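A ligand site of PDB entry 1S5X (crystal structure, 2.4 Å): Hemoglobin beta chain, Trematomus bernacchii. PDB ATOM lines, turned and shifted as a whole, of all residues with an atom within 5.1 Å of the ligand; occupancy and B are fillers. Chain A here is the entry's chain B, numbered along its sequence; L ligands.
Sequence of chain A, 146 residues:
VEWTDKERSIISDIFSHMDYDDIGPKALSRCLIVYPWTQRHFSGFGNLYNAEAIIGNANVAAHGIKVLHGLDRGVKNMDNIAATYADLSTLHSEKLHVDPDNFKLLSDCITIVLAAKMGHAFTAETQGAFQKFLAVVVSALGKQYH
A ring nitrogen (NE2) of His 92 binds an iron atom (FE1) of the ligand. A ring nitrogen (NE2) of His 63 is bound to an iron atom (FE1) of the ligand (2.0 Å). O3 of the ligand lies within salt-bridge range of NZ of Lys 66 (3.1 Å).
A ring nitrogen (ND1) of His 92 lies within hydrogen-bond range of the backbone carbonyl oxygen (O) of Leu 88, 2.8 Å away. The backbone carbonyl oxygen (O) of His 92 sits at hydrogen-bond distance from the backbone NH (N) of Val 98. A ring nitrogen (NE2) of His 41 lies within hydrogen-bond range of the side-chain amide nitrogen of Asn 102. N of Leu 96 lies within hydrogen-bond range of O of Leu 91, 2.9 Å away.
Merely in contact with the ligand: Thr 38, His 41, Phe 42, Val 67, Leu 88, Leu 91, Leu 96, Val 98, Asn 102, Phe 103, Leu 106 and Leu 141. Hydrophobic or aromatic side chains within 4 Å of the ligand: His 41, Phe 42, His 63, Val 67, Leu 88, Leu 91, His 92, Leu 96, Val 98, Phe 103, Leu 106 and Leu 141. Within 4 Å of the ligand: Thr 38, His 41, Phe 42, His 63, Lys 66, Val 67, Leu 88, Leu 91, His 92, Leu 96, Val 98, Asn 102, Phe 103, Leu 106 and Leu 141. Along chain A the residues within 4 Å of the ligand span positions 38 to 141.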
ATOM      1  N   LEU A  28      12.246  23.933 -25.532  1.00  0.00           N
ATOM      2  CA  LEU A  28      10.964  23.731 -26.232  1.00  0.00           C
ATOM      3  C   LEU A  28      11.196  23.170 -27.643  1.00  0.00           C
ATOM      4  O   LEU A  28      10.509  22.251 -28.070  1.00  0.00           O
ATOM      5  CB  LEU A  28      10.137  25.037 -26.283  1.00  0.00           C
ATOM      6  CG  LEU A  28       8.684  24.906 -26.778  1.00  0.00           C
ATOM      7  CD1 LEU A  28       7.925  23.936 -25.892  1.00  0.00           C
ATOM      8  CD2 LEU A  28       7.985  26.289 -26.787  1.00  0.00           C
ATOM      9  N   LEU A  32       9.810  19.695 -29.258  1.00  0.00           N
ATOM     10  CA  LEU A  32       8.996  19.635 -30.459  1.00  0.00           C
ATOM     11  C   LEU A  32       9.618  18.731 -31.494  1.00  0.00           C
ATOM     12  O   LEU A  32       8.910  18.130 -32.279  1.00  0.00           O
ATOM     13  CB  LEU A  32       8.751  21.025 -31.040  1.00  0.00           C
ATOM     14  CG  LEU A  32       7.917  21.998 -30.176  1.00  0.00           C
ATOM     15  CD1 LEU A  32       7.227  23.024 -31.060  1.00  0.00           C
ATOM     16  CD2 LEU A  32       6.879  21.230 -29.385  1.00  0.00           C
ATOM     17  N   THR A  38       3.878  17.107 -30.063  1.00  0.00           N
ATOM     18  CA  THR A  38       3.653  18.289 -29.244  1.00  0.00           C
ATOM     19  C   THR A  38       3.612  19.522 -30.148  1.00  0.00           C
ATOM     20  O   THR A  38       3.180  20.597 -29.724  1.00  0.00           O
ATOM     21  CB  THR A  38       4.777  18.467 -28.168  1.00  0.00           C
ATOM     22  OG1 THR A  38       6.056  18.467 -28.810  1.00  0.00           O
ATOM     23  CG2 THR A  38       4.726  17.336 -27.148  1.00  0.00           C
ATOM     24  N   HIS A  41       0.292  21.945 -30.813  1.00  0.00           N
ATOM     25  CA  HIS A  41      -0.113  23.073 -29.967  1.00  0.00           C
ATOM     26  C   HIS A  41       0.524  24.371 -30.454  1.00  0.00           C
ATOM     27  O   HIS A  41       0.250  25.434 -29.903  1.00  0.00           O
ATOM     28  CB  HIS A  41       0.282  22.789 -28.510  1.00  0.00           C
ATOM     29  CG  HIS A  41      -0.271  21.506 -27.986  1.00  0.00           C
ATOM     30  ND1 HIS A  41      -1.583  21.366 -27.580  1.00  0.00           N
ATOM     31  CD2 HIS A  41       0.308  20.298 -27.795  1.00  0.00           C
ATOM     32  CE1 HIS A  41      -1.791  20.124 -27.166  1.00  0.00           C
ATOM     33  NE2 HIS A  41      -0.657  19.453 -27.294  1.00  0.00           N
ATOM     34  N   PHE A  42       1.361  24.279 -31.480  1.00  0.00           N
ATOM     35  CA  PHE A  42       2.043  25.436 -32.043  1.00  0.00           C
ATOM     36  C   PHE A  42       1.858  25.573 -33.563  1.00  0.00           C
ATOM     37  O   PHE A  42       2.694  26.141 -34.255  1.00  0.00           O
ATOM     38  CB  PHE A  42       3.542  25.372 -31.710  1.00  0.00           C
ATOM     39  CG  PHE A  42       3.811  25.430 -30.242  1.00  0.00           C
ATOM     40  CD1 PHE A  42       3.903  26.649 -29.576  1.00  0.00           C
ATOM     41  CD2 PHE A  42       3.876  24.261 -29.491  1.00  0.00           C
ATOM     42  CE1 PHE A  42       4.039  26.703 -28.205  1.00  0.00           C
ATOM     43  CE2 PHE A  42       4.013  24.298 -28.120  1.00  0.00           C
ATOM     44  CZ  PHE A  42       4.094  25.521 -27.473  1.00  0.00           C
ATOM     45  N   ASN A  59       7.843  32.202 -32.229  1.00  0.00           N
ATOM     46  CA  ASN A  59       6.689  31.910 -31.368  1.00  0.00           C
ATOM     47  C   ASN A  59       7.069  30.795 -30.405  1.00  0.00           C
ATOM     48  O   ASN A  59       6.711  30.811 -29.231  1.00  0.00           O
ATOM     49  CB  ASN A  59       5.461  31.481 -32.180  1.00  0.00           C
ATOM     50  CG  ASN A  59       5.007  32.541 -33.175  1.00  0.00           C
ATOM     51  OD1 ASN A  59       4.801  33.703 -32.802  1.00  0.00           O
ATOM     52  ND2 ASN A  59       4.836  32.154 -34.444  1.00  0.00           N
ATOM     53  N   HIS A  63       7.361  31.183 -26.158  1.00  0.00           N
ATOM     54  CA  HIS A  63       6.768  30.290 -25.168  1.00  0.00           C
ATOM     55  C   HIS A  63       7.856  29.538 -24.394  1.00  0.00           C
ATOM     56  O   HIS A  63       7.658  29.176 -23.234  1.00  0.00           O
ATOM     57  CB  HIS A  63       5.826  29.266 -25.816  1.00  0.00           C
ATOM     58  CG  HIS A  63       5.166  28.337 -24.831  1.00  0.00           C
ATOM     59  ND1 HIS A  63       5.570  27.047 -24.592  1.00  0.00           N
ATOM     60  CD2 HIS A  63       4.151  28.570 -23.968  1.00  0.00           C
ATOM     61  CE1 HIS A  63       4.802  26.548 -23.591  1.00  0.00           C
ATOM     62  NE2 HIS A  63       3.915  27.423 -23.176  1.00  0.00           N
ATOM     63  N   LYS A  66       8.691  31.761 -21.622  1.00  0.00           N
ATOM     64  CA  LYS A  66       7.592  31.824 -20.647  1.00  0.00           C
ATOM     65  C   LYS A  66       7.586  30.627 -19.706  1.00  0.00           C
ATOM     66  O   LYS A  66       7.163  30.741 -18.545  1.00  0.00           O
ATOM     67  CB  LYS A  66       6.261  31.913 -21.366  1.00  0.00           C
ATOM     68  CG  LYS A  66       6.044  33.229 -22.088  1.00  0.00           C
ATOM     69  CD  LYS A  66       4.690  33.240 -22.796  1.00  0.00           C
ATOM     70  CE  LYS A  66       4.462  34.584 -23.477  1.00  0.00           C
ATOM     71  NZ  LYS A  66       3.353  34.518 -24.466  1.00  0.00           N
ATOM     72  N   VAL A  67       8.032  29.467 -20.191  1.00  0.00           N
ATOM     73  CA  VAL A  67       8.068  28.273 -19.354  1.00  0.00           C
ATOM     74  C   VAL A  67       9.071  28.502 -18.210  1.00  0.00           C
ATOM     75  O   VAL A  67       8.805  28.169 -17.050  1.00  0.00           O
ATOM     76  CB  VAL A  67       8.514  27.027 -20.156  1.00  0.00           C
ATOM     77  CG1 VAL A  67       8.925  25.915 -19.211  1.00  0.00           C
ATOM     78  CG2 VAL A  67       7.389  26.566 -21.068  1.00  0.00           C
ATOM     79  N   GLY A  70       7.768  30.815 -15.712  1.00  0.00           N
ATOM     80  CA  GLY A  70       6.749  30.148 -14.924  1.00  0.00           C
ATOM     81  C   GLY A  70       7.357  29.261 -13.847  1.00  0.00           C
ATOM     82  O   GLY A  70       6.870  29.217 -12.716  1.00  0.00           O
ATOM     83  N   LEU A  71       8.425  28.539 -14.197  1.00  0.00           N
ATOM     84  CA  LEU A  71       9.097  27.658 -13.232  1.00  0.00           C
ATOM     85  C   LEU A  71       9.741  28.511 -12.152  1.00  0.00           C
ATOM     86  O   LEU A  71       9.900  28.083 -10.997  1.00  0.00           O
ATOM     87  CB  LEU A  71      10.190  26.848 -13.914  1.00  0.00           C
ATOM     88  CG  LEU A  71       9.762  25.833 -14.969  1.00  0.00           C
ATOM     89  CD1 LEU A  71      10.965  25.009 -15.359  1.00  0.00           C
ATOM     90  CD2 LEU A  71       8.667  24.928 -14.398  1.00  0.00           C
ATOM     91  N   TYR A  85       0.357  27.205  -9.219  1.00  0.00           N
ATOM     92  CA  TYR A  85       0.088  26.887 -10.615  1.00  0.00           C
ATOM     93  C   TYR A  85      -1.370  26.606 -11.004  1.00  0.00           C
ATOM     94  O   TYR A  85      -1.637  26.205 -12.150  1.00  0.00           O
ATOM     95  CB  TYR A  85       0.976  25.722 -11.062  1.00  0.00           C
ATOM     96  CG  TYR A  85       2.461  26.035 -11.079  1.00  0.00           C
ATOM     97  CD1 TYR A  85       3.321  25.475 -10.140  1.00  0.00           C
ATOM     98  CD2 TYR A  85       2.990  26.904 -12.032  1.00  0.00           C
ATOM     99  CE1 TYR A  85       4.677  25.764 -10.150  1.00  0.00           C
ATOM    100  CE2 TYR A  85       4.346  27.204 -12.049  1.00  0.00           C
ATOM    101  CZ  TYR A  85       5.181  26.624 -11.116  1.00  0.00           C
ATOM    102  OH  TYR A  85       6.518  26.911 -11.142  1.00  0.00           O
ATOM    103  N   LEU A  88      -2.334  28.376 -14.282  1.00  0.00           N
ATOM    104  CA  LEU A  88      -1.698  27.785 -15.448  1.00  0.00           C
ATOM    105  C   LEU A  88      -2.235  26.400 -15.791  1.00  0.00           C
ATOM    106  O   LEU A  88      -2.341  26.044 -16.964  1.00  0.00           O
ATOM    107  CB  LEU A  88      -0.180  27.710 -15.241  1.00  0.00           C
ATOM    108  CG  LEU A  88       0.579  29.026 -15.292  1.00  0.00           C
ATOM    109  CD1 LEU A  88       2.036  28.749 -14.920  1.00  0.00           C
ATOM    110  CD2 LEU A  88       0.469  29.643 -16.681  1.00  0.00           C
ATOM    111  N   LEU A  91      -5.559  26.667 -17.488  1.00  0.00           N
ATOM    112  CA  LEU A  91      -5.312  27.212 -18.815  1.00  0.00           C
ATOM    113  C   LEU A  91      -4.825  26.183 -19.836  1.00  0.00           C
ATOM    114  O   LEU A  91      -5.381  26.100 -20.936  1.00  0.00           O
ATOM    115  CB  LEU A  91      -4.287  28.360 -18.761  1.00  0.00           C
ATOM    116  CG  LEU A  91      -3.872  28.905 -20.131  1.00  0.00           C
ATOM    117  CD1 LEU A  91      -4.962  29.787 -20.708  1.00  0.00           C
ATOM    118  CD2 LEU A  91      -2.586  29.699 -19.991  1.00  0.00           C
ATOM    119  N   HIS A  92      -3.785  25.432 -19.480  1.00  0.00           N
ATOM    120  CA  HIS A  92      -3.219  24.436 -20.401  1.00  0.00           C
ATOM    121  C   HIS A  92      -4.160  23.243 -20.564  1.00  0.00           C
ATOM    122  O   HIS A  92      -4.246  22.635 -21.626  1.00  0.00           O
ATOM    123  CB  HIS A  92      -1.847  23.942 -19.923  1.00  0.00           C
ATOM    124  CG  HIS A  92      -0.758  24.962 -20.049  1.00  0.00           C
ATOM    125  ND1 HIS A  92      -0.558  26.009 -19.180  1.00  0.00           N
ATOM    126  CD2 HIS A  92       0.192  25.109 -21.013  1.00  0.00           C
ATOM    127  CE1 HIS A  92       0.472  26.735 -19.616  1.00  0.00           C
ATOM    128  NE2 HIS A  92       0.965  26.228 -20.730  1.00  0.00           N
ATOM    129  N   LEU A  96      -6.345  25.074 -23.491  1.00  0.00           N
ATOM    130  CA  LEU A  96      -5.349  24.778 -24.516  1.00  0.00           C
ATOM    131  C   LEU A  96      -5.352  23.292 -24.930  1.00  0.00           C
ATOM    132  O   LEU A  96      -4.885  22.951 -26.006  1.00  0.00           O
ATOM    133  CB  LEU A  96      -3.961  25.192 -24.027  1.00  0.00           C
ATOM    134  CG  LEU A  96      -3.386  26.566 -24.384  1.00  0.00           C
ATOM    135  CD1 LEU A  96      -4.437  27.632 -24.527  1.00  0.00           C
ATOM    136  CD2 LEU A  96      -2.409  26.938 -23.298  1.00  0.00           C
ATOM    137  N   VAL A  98      -3.727  20.576 -23.640  1.00  0.00           N
ATOM    138  CA  VAL A  98      -2.422  19.959 -23.671  1.00  0.00           C
ATOM    139  C   VAL A  98      -2.495  18.701 -22.832  1.00  0.00           C
ATOM    140  O   VAL A  98      -2.875  18.750 -21.674  1.00  0.00           O
ATOM    141  CB  VAL A  98      -1.350  20.898 -23.077  1.00  0.00           C
ATOM    142  CG1 VAL A  98      -0.024  20.152 -22.923  1.00  0.00           C
ATOM    143  CG2 VAL A  98      -1.172  22.120 -23.988  1.00  0.00           C
ATOM    144  N   ASN A 102       2.497  15.489 -21.911  1.00  0.00           N
ATOM    145  CA  ASN A 102       3.393  16.453 -22.566  1.00  0.00           C
ATOM    146  C   ASN A 102       4.287  17.216 -21.568  1.00  0.00           C
ATOM    147  O   ASN A 102       5.353  17.684 -21.936  1.00  0.00           O
ATOM    148  CB  ASN A 102       2.583  17.467 -23.387  1.00  0.00           C
ATOM    149  CG  ASN A 102       1.859  16.836 -24.584  1.00  0.00           C
ATOM    150  OD1 ASN A 102       1.863  15.615 -24.781  1.00  0.00           O
ATOM    151  ND2 ASN A 102       1.207  17.675 -25.374  1.00  0.00           N
ATOM    152  N   PHE A 103       3.845  17.340 -20.318  1.00  0.00           N
ATOM    153  CA  PHE A 103       4.648  18.053 -19.309  1.00  0.00           C
ATOM    154  C   PHE A 103       5.837  17.225 -18.895  1.00  0.00           C
ATOM    155  O   PHE A 103       6.895  17.788 -18.615  1.00  0.00           O
ATOM    156  CB  PHE A 103       3.815  18.386 -18.063  1.00  0.00           C
ATOM    157  CG  PHE A 103       2.742  19.395 -18.324  1.00  0.00           C
ATOM    158  CD1 PHE A 103       3.078  20.656 -18.804  1.00  0.00           C
ATOM    159  CD2 PHE A 103       1.403  19.052 -18.183  1.00  0.00           C
ATOM    160  CE1 PHE A 103       2.084  21.563 -19.145  1.00  0.00           C
ATOM    161  CE2 PHE A 103       0.416  19.954 -18.519  1.00  0.00           C
ATOM    162  CZ  PHE A 103       0.753  21.209 -19.007  1.00  0.00           C
ATOM    163  N   LEU A 106       8.363  17.505 -21.811  1.00  0.00           N
ATOM    164  CA  LEU A 106       9.062  18.803 -21.841  1.00  0.00           C
ATOM    165  C   LEU A 106      10.043  18.915 -20.669  1.00  0.00           C
ATOM    166  O   LEU A 106      11.105  19.531 -20.766  1.00  0.00           O
ATOM    167  CB  LEU A 106       8.047  19.974 -21.784  1.00  0.00           C
ATOM    168  CG  LEU A 106       8.644  21.375 -21.538  1.00  0.00           C
ATOM    169  CD1 LEU A 106       9.581  21.734 -22.656  1.00  0.00           C
ATOM    170  CD2 LEU A 106       7.555  22.428 -21.443  1.00  0.00           C
ATOM    171  N   ILE A 110      14.189  19.894 -20.654  1.00  0.00           N
ATOM    172  CA  ILE A 110      14.766  20.997 -19.923  1.00  0.00           C
ATOM    173  C   ILE A 110      16.004  20.428 -19.202  1.00  0.00           C
ATOM    174  O   ILE A 110      17.081  21.006 -19.243  1.00  0.00           O
ATOM    175  CB  ILE A 110      13.752  21.564 -18.882  1.00  0.00           C
ATOM    176  CG1 ILE A 110      12.497  22.090 -19.603  1.00  0.00           C
ATOM    177  CG2 ILE A 110      14.410  22.705 -18.068  1.00  0.00           C
ATOM    178  CD1 ILE A 110      11.376  22.563 -18.663  1.00  0.00           C
ATOM    179  N   LEU A 141       0.665  20.909 -12.648  1.00  0.00           N
ATOM    180  CA  LEU A 141       0.168  21.323 -13.949  1.00  0.00           C
ATOM    181  C   LEU A 141      -0.736  20.273 -14.594  1.00  0.00           C
ATOM    182  O   LEU A 141      -1.623  20.600 -15.386  1.00  0.00           O
ATOM    183  CB  LEU A 141       1.342  21.674 -14.871  1.00  0.00           C
ATOM    184  CG  LEU A 141       1.963  23.050 -14.587  1.00  0.00           C
ATOM    185  CD1 LEU A 141       3.292  23.170 -15.289  1.00  0.00           C
ATOM    186  CD2 LEU A 141       1.004  24.151 -15.032  1.00  0.00           C
HETATM  187  C1  LIG L   1       1.054  29.395 -22.764  1.00  0.00           C
HETATM  188  C2  LIG L   1       3.782  28.194 -19.042  1.00  0.00           C
HETATM  189  C3  LIG L   1       4.110  23.750 -20.765  1.00  0.00           C
HETATM  190  C4  LIG L   1       1.575  24.974 -24.703  1.00  0.00           C
HETATM  191  C5  LIG L   1       1.739  29.516 -21.567  1.00  0.00           C
HETATM  192  C6  LIG L   1       1.889  30.721 -20.748  1.00  0.00           C
HETATM  193  C7  LIG L   1       2.704  30.366 -19.692  1.00  0.00           C
HETATM  194  C8  LIG L   1       3.009  28.962 -19.878  1.00  0.00           C
HETATM  195  C9  LIG L   1       3.220  31.241 -18.563  1.00  0.00           C
HETATM  196  C10 LIG L   1       1.309  32.095 -21.058  1.00  0.00           C
HETATM  197  C11 LIG L   1      -0.126  32.189 -20.450  1.00  0.00           C
HETATM  198  C12 LIG L   1      -0.929  33.319 -20.785  1.00  0.00           C
HETATM  199  O1  LIG L   1      -1.994  33.558 -20.002  1.00  0.00           O
HETATM  200  O2  LIG L   1      -0.643  34.087 -21.733  1.00  0.00           O
HETATM  201  C13 LIG L   1       4.097  26.862 -19.138  1.00  0.00           C
HETATM  202  C14 LIG L   1       4.815  26.149 -18.092  1.00  0.00           C
HETATM  203  C15 LIG L   1       4.895  24.857 -18.558  1.00  0.00           C
HETATM  204  C16 LIG L   1       4.241  24.842 -19.897  1.00  0.00           C
HETATM  205  C17 LIG L   1       5.341  26.721 -16.705  1.00  0.00           C
HETATM  206  C18 LIG L   1       5.527  23.744 -17.740  1.00  0.00           C
HETATM  207  C19 LIG L   1       6.709  22.888 -18.152  1.00  0.00           C
HETATM  208  C20 LIG L   1       3.510  23.631 -21.991  1.00  0.00           C
HETATM  209  C21 LIG L   1       3.481  22.451 -22.882  1.00  0.00           C
HETATM  210  C22 LIG L   1       2.754  22.825 -23.991  1.00  0.00           C
HETATM  211  C23 LIG L   1       2.345  24.189 -23.805  1.00  0.00           C
HETATM  212  C24 LIG L   1       4.154  21.097 -22.612  1.00  0.00           C
HETATM  213  C25 LIG L   1       2.426  21.975 -25.237  1.00  0.00           C
HETATM  214  C26 LIG L   1       3.669  21.533 -26.078  1.00  0.00           C
HETATM  215  C27 LIG L   1       1.161  26.314 -24.552  1.00  0.00           C
HETATM  216  C28 LIG L   1       0.418  27.106 -25.548  1.00  0.00           C
HETATM  217  C29 LIG L   1       0.297  28.354 -24.999  1.00  0.00           C
HETATM  218  C30 LIG L   1       0.924  28.302 -23.669  1.00  0.00           C
HETATM  219  C31 LIG L   1      -0.046  26.571 -26.905  1.00  0.00           C
HETATM  220  C32 LIG L   1      -0.280  29.634 -25.530  1.00  0.00           C
HETATM  221  C33 LIG L   1       0.701  30.463 -26.507  1.00  0.00           C
HETATM  222  C34 LIG L   1       1.720  31.326 -25.973  1.00  0.00           C
HETATM  223  O3  LIG L   1       1.441  32.161 -25.022  1.00  0.00           O
HETATM  224  O4  LIG L   1       2.890  31.386 -26.462  1.00  0.00           O
HETATM  225  N1  LIG L   1       2.426  28.463 -21.054  1.00  0.00           N
HETATM  226  N2  LIG L   1       3.708  26.083 -20.224  1.00  0.00           N
HETATM  227  N3  LIG L   1       2.818  24.701 -22.592  1.00  0.00           N
HETATM  228  N4  LIG L   1       1.488  27.081 -23.436  1.00  0.00           N
HETATM  229 FE1  LIG L   1       2.604  26.591 -21.848  1.00  0.00          FE
